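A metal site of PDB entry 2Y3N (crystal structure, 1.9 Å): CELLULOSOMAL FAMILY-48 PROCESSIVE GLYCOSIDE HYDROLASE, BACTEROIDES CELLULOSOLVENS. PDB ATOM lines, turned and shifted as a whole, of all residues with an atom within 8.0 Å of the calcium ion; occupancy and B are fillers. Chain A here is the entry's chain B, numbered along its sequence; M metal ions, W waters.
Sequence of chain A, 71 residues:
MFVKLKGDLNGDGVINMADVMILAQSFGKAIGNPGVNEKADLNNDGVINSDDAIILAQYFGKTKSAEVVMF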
ATOM      1  N   LEU A  23     -35.699  -5.058  14.687  1.00  0.00           N
ATOM      2  CA  LEU A  23     -34.317  -5.414  14.666  1.00  0.00           C
ATOM      3  C   LEU A  23     -33.542  -4.370  15.521  1.00  0.00           C
ATOM      4  O   LEU A  23     -32.767  -4.728  16.426  1.00  0.00           O
ATOM      5  CB  LEU A  23     -33.804  -5.437  13.222  1.00  0.00           C
ATOM      6  CG  LEU A  23     -32.667  -6.325  12.793  1.00  0.00           C
ATOM      7  CD1 LEU A  23     -32.740  -6.591  11.297  1.00  0.00           C
ATOM      8  CD2 LEU A  23     -31.320  -5.701  13.172  1.00  0.00           C
ATOM      9  N   LYS A  29     -27.551  -6.953  20.641  1.00  0.00           N
ATOM     10  CA  LYS A  29     -27.840  -7.862  21.741  1.00  0.00           C
ATOM     11  C   LYS A  29     -27.610  -9.292  21.354  1.00  0.00           C
ATOM     12  O   LYS A  29     -27.927  -9.675  20.224  1.00  0.00           O
ATOM     13  CB  LYS A  29     -29.280  -7.706  22.191  1.00  0.00           C
ATOM     14  CG  LYS A  29     -29.635  -6.365  22.788  1.00  0.00           C
ATOM     15  CD  LYS A  29     -28.748  -6.030  23.953  1.00  0.00           C
ATOM     16  CE  LYS A  29     -29.534  -5.282  25.024  1.00  0.00           C
ATOM     17  NZ  LYS A  29     -29.876  -3.904  24.544  1.00  0.00           N
ATOM     18  N   GLU A  38     -35.345 -13.255  19.372  1.00  0.00           N
ATOM     19  CA  GLU A  38     -34.870 -14.464  18.681  1.00  0.00           C
ATOM     20  C   GLU A  38     -35.291 -14.507  17.206  1.00  0.00           C
ATOM     21  O   GLU A  38     -34.488 -14.945  16.360  1.00  0.00           O
ATOM     22  CB  GLU A  38     -35.246 -15.763  19.434  1.00  0.00           C
ATOM     23  CG  GLU A  38     -36.747 -16.130  19.547  1.00  0.00           C
ATOM     24  CD  GLU A  38     -37.000 -17.161  20.660  1.00  0.00           C
ATOM     25  OE1 GLU A  38     -36.031 -17.543  21.356  1.00  0.00           O
ATOM     26  OE2 GLU A  38     -38.155 -17.611  20.849  1.00  0.00           O
ATOM     27  N   ALA A  40     -35.479 -11.939  15.382  1.00  0.00           N
ATOM     28  CA  ALA A  40     -34.707 -10.889  14.728  1.00  0.00           C
ATOM     29  C   ALA A  40     -33.297 -11.412  14.361  1.00  0.00           C
ATOM     30  O   ALA A  40     -32.597 -10.791  13.560  1.00  0.00           O
ATOM     31  CB  ALA A  40     -34.633  -9.666  15.629  1.00  0.00           C
ATOM     32  N   ASP A  41     -32.907 -12.561  14.941  1.00  0.00           N
ATOM     33  CA  ASP A  41     -31.662 -13.195  14.577  1.00  0.00           C
ATOM     34  C   ASP A  41     -31.801 -13.910  13.266  1.00  0.00           C
ATOM     35  O   ASP A  41     -31.797 -15.141  13.209  1.00  0.00           O
ATOM     36  CB  ASP A  41     -31.170 -14.138  15.671  1.00  0.00           C
ATOM     37  CG  ASP A  41     -29.793 -14.666  15.377  1.00  0.00           C
ATOM     38  OD1 ASP A  41     -29.145 -14.180  14.434  1.00  0.00           O
ATOM     39  OD2 ASP A  41     -29.379 -15.593  16.074  1.00  0.00           O
ATOM     40  N   LEU A  42     -31.808 -13.126  12.216  1.00  0.00           N
ATOM     41  CA  LEU A  42     -32.194 -13.584  10.899  1.00  0.00           C
ATOM     42  C   LEU A  42     -31.202 -14.562  10.239  1.00  0.00           C
ATOM     43  O   LEU A  42     -31.599 -15.380   9.455  1.00  0.00           O
ATOM     44  CB  LEU A  42     -32.440 -12.388  10.018  1.00  0.00           C
ATOM     45  CG  LEU A  42     -33.764 -11.624  10.260  1.00  0.00           C
ATOM     46  CD1 LEU A  42     -33.759 -10.340   9.461  1.00  0.00           C
ATOM     47  CD2 LEU A  42     -35.011 -12.431   9.968  1.00  0.00           C
ATOM     48  N   ASN A  43     -29.951 -14.541  10.640  1.00  0.00           N
ATOM     49  CA  ASN A  43     -28.977 -15.536  10.149  1.00  0.00           C
ATOM     50  C   ASN A  43     -28.660 -16.553  11.206  1.00  0.00           C
ATOM     51  O   ASN A  43     -27.772 -17.386  11.034  1.00  0.00           O
ATOM     52  CB  ASN A  43     -27.684 -14.876   9.679  1.00  0.00           C
ATOM     53  CG  ASN A  43     -27.010 -14.037  10.778  1.00  0.00           C
ATOM     54  OD1 ASN A  43     -27.448 -14.030  11.934  1.00  0.00           O
ATOM     55  ND2 ASN A  43     -25.954 -13.344  10.411  1.00  0.00           N
ATOM     56  N   ASN A  44     -29.320 -16.448  12.347  1.00  0.00           N
ATOM     57  CA  ASN A  44     -29.196 -17.468  13.340  1.00  0.00           C
ATOM     58  C   ASN A  44     -27.815 -17.660  13.938  1.00  0.00           C
ATOM     59  O   ASN A  44     -27.465 -18.753  14.353  1.00  0.00           O
ATOM     60  CB  ASN A  44     -29.728 -18.778  12.765  1.00  0.00           C
ATOM     61  CG  ASN A  44     -31.248 -18.889  12.906  1.00  0.00           C
ATOM     62  OD1 ASN A  44     -31.829 -18.389  13.875  1.00  0.00           O
ATOM     63  ND2 ASN A  44     -31.886 -19.550  11.953  1.00  0.00           N
ATOM     64  N   ASP A  45     -27.009 -16.592  13.971  1.00  0.00           N
ATOM     65  CA  ASP A  45     -25.654 -16.709  14.527  1.00  0.00           C
ATOM     66  C   ASP A  45     -25.541 -16.297  15.998  1.00  0.00           C
ATOM     67  O   ASP A  45     -24.447 -16.011  16.469  1.00  0.00           O
ATOM     68  CB  ASP A  45     -24.628 -15.927  13.703  1.00  0.00           C
ATOM     69  CG  ASP A  45     -24.877 -14.417  13.751  1.00  0.00           C
ATOM     70  OD1 ASP A  45     -25.841 -14.022  14.430  1.00  0.00           O
ATOM     71  OD2 ASP A  45     -24.100 -13.669  13.125  1.00  0.00           O
ATOM     72  N   GLY A  46     -26.671 -16.266  16.721  1.00  0.00           N
ATOM     73  CA  GLY A  46     -26.679 -15.978  18.170  1.00  0.00           C
ATOM     74  C   GLY A  46     -26.703 -14.483  18.518  1.00  0.00           C
ATOM     75  O   GLY A  46     -26.894 -14.128  19.684  1.00  0.00           O
ATOM     76  N   VAL A  47     -26.545 -13.618  17.511  1.00  0.00           N
ATOM     77  CA  VAL A  47     -26.421 -12.168  17.732  1.00  0.00           C
ATOM     78  C   VAL A  47     -27.258 -11.330  16.754  1.00  0.00           C
ATOM     79  O   VAL A  47     -27.462 -11.719  15.614  1.00  0.00           O
ATOM     80  CB  VAL A  47     -24.904 -11.720  17.760  1.00  0.00           C
ATOM     81  CG1 VAL A  47     -24.359 -11.579  16.351  1.00  0.00           C
ATOM     82  CG2 VAL A  47     -24.712 -10.438  18.531  1.00  0.00           C
ATOM     83  N   ILE A  48     -27.757 -10.187  17.233  1.00  0.00           N
ATOM     84  CA  ILE A  48     -28.530  -9.226  16.383  1.00  0.00           C
ATOM     85  C   ILE A  48     -27.577  -8.101  15.986  1.00  0.00           C
ATOM     86  O   ILE A  48     -27.136  -7.329  16.843  1.00  0.00           O
ATOM     87  CB  ILE A  48     -29.722  -8.591  17.180  1.00  0.00           C
ATOM     88  CG1 ILE A  48     -30.720  -9.680  17.634  1.00  0.00           C
ATOM     89  CG2 ILE A  48     -30.483  -7.484  16.352  1.00  0.00           C
ATOM     90  CD1 ILE A  48     -31.035 -10.582  16.536  1.00  0.00           C
ATOM     91  N   ASN A  49     -27.185  -8.046  14.710  1.00  0.00           N
ATOM     92  CA  ASN A  49     -26.405  -6.893  14.265  1.00  0.00           C
ATOM     93  C   ASN A  49     -26.642  -6.531  12.793  1.00  0.00           C
ATOM     94  O   ASN A  49     -27.606  -7.026  12.198  1.00  0.00           O
ATOM     95  CB  ASN A  49     -24.921  -7.145  14.499  1.00  0.00           C
ATOM     96  CG  ASN A  49     -24.387  -8.345  13.696  1.00  0.00           C
ATOM     97  OD1 ASN A  49     -25.084  -8.901  12.861  1.00  0.00           O
ATOM     98  ND2 ASN A  49     -23.125  -8.695  13.917  1.00  0.00           N
ATOM     99  N   SER A  50     -25.715  -5.815  12.166  1.00  0.00           N
ATOM    100  CA  SER A  50     -25.960  -5.385  10.791  1.00  0.00           C
ATOM    101  C   SER A  50     -26.119  -6.547   9.828  1.00  0.00           C
ATOM    102  O   SER A  50     -26.661  -6.334   8.763  1.00  0.00           O
ATOM    103  CB  SER A  50     -24.819  -4.495  10.270  1.00  0.00           C
ATOM    104  OG  SER A  50     -24.832  -3.278  11.008  1.00  0.00           O
ATOM    105  N   ASP A  51     -25.565  -7.731  10.118  1.00  0.00           N
ATOM    106  CA  ASP A  51     -25.755  -8.854   9.185  1.00  0.00           C
ATOM    107  C   ASP A  51     -27.263  -9.105   9.033  1.00  0.00           C
ATOM    108  O   ASP A  51     -27.776  -9.390   7.915  1.00  0.00           O
ATOM    109  CB  ASP A  51     -25.145 -10.168   9.681  1.00  0.00           C
ATOM    110  CG  ASP A  51     -23.634 -10.192   9.573  1.00  0.00           C
ATOM    111  OD1 ASP A  51     -23.074  -9.389   8.816  1.00  0.00           O
ATOM    112  OD2 ASP A  51     -23.023 -10.989  10.270  1.00  0.00           O
ATOM    113  N   ASP A  52     -27.958  -9.061  10.164  1.00  0.00           N
ATOM    114  CA  ASP A  52     -29.435  -9.264  10.165  1.00  0.00           C
ATOM    115  C   ASP A  52     -30.141  -8.134   9.386  1.00  0.00           C
ATOM    116  O   ASP A  52     -31.040  -8.415   8.586  1.00  0.00           O
ATOM    117  CB  ASP A  52     -29.912  -9.326  11.585  1.00  0.00           C
ATOM    118  CG  ASP A  52     -29.195 -10.443  12.368  1.00  0.00           C
ATOM    119  OD1 ASP A  52     -29.448 -11.607  12.058  1.00  0.00           O
ATOM    120  OD2 ASP A  52     -28.345 -10.123  13.246  1.00  0.00           O
ATOM    121  N   ALA A  53     -29.696  -6.888   9.569  1.00  0.00           N
ATOM    122  CA  ALA A  53     -30.151  -5.773   8.738  1.00  0.00           C
ATOM    123  C   ALA A  53     -29.867  -5.954   7.226  1.00  0.00           C
ATOM    124  O   ALA A  53     -30.687  -5.571   6.360  1.00  0.00           O
ATOM    125  CB  ALA A  53     -29.573  -4.410   9.243  1.00  0.00           C
ATOM    126  N   ILE A  55     -29.635  -8.824   5.643  1.00  0.00           N
ATOM    127  CA  ILE A  55     -30.529  -9.874   5.211  1.00  0.00           C
ATOM    128  C   ILE A  55     -31.882  -9.242   4.980  1.00  0.00           C
ATOM    129  O   ILE A  55     -32.467  -9.371   3.906  1.00  0.00           O
ATOM    130  CB  ILE A  55     -30.654 -11.027   6.275  1.00  0.00           C
ATOM    131  CG1 ILE A  55     -29.405 -11.885   6.250  1.00  0.00           C
ATOM    132  CG2 ILE A  55     -31.889 -11.913   5.979  1.00  0.00           C
ATOM    133  CD1 ILE A  55     -29.403 -13.000   7.372  1.00  0.00           C
HETATM  134 CA    CA M   1     -27.498 -12.501  13.552  1.00  0.00          CA
HETATM  135  O   HOH W   1     -25.582 -11.336  12.881  1.00  0.00           O
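Water W1 lies within hydrogen-bond range of the side-chain amide oxygen of Asn 49 (2.5 Å), the side-chain carboxylate of Asp 45 (2.8 Å) and the side-chain amide nitrogen of Asn 43 (3.2 Å).
The side-chain carboxylate of Asp 52 sits close to the backbone NH of Asn 49, at 2.8 Å.
OD2 of Asp 41 sits at hydrogen-bond distance from N of Gly 46 (2.9 Å).
The backbone carbonyl oxygen of Asp 41 lies close to the side-chain amide oxygen of Asn 44, at 3.3 Å.
The backbone NH of Leu 42 lies close to the side-chain carboxylate of Asp 52 (2.8 Å).
The calcium ion is bound by O of Val 47, OD1 of Asn 43, water W1, OD1 of Asp 45, OD1 of Asp 41, OD2 of Asp 52 and OD1 of Asp 52.
The calcium ion has seven donor atoms within binding distance.
Of the 18 residues printed, 5 come within 4 Å of the calcium ion.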
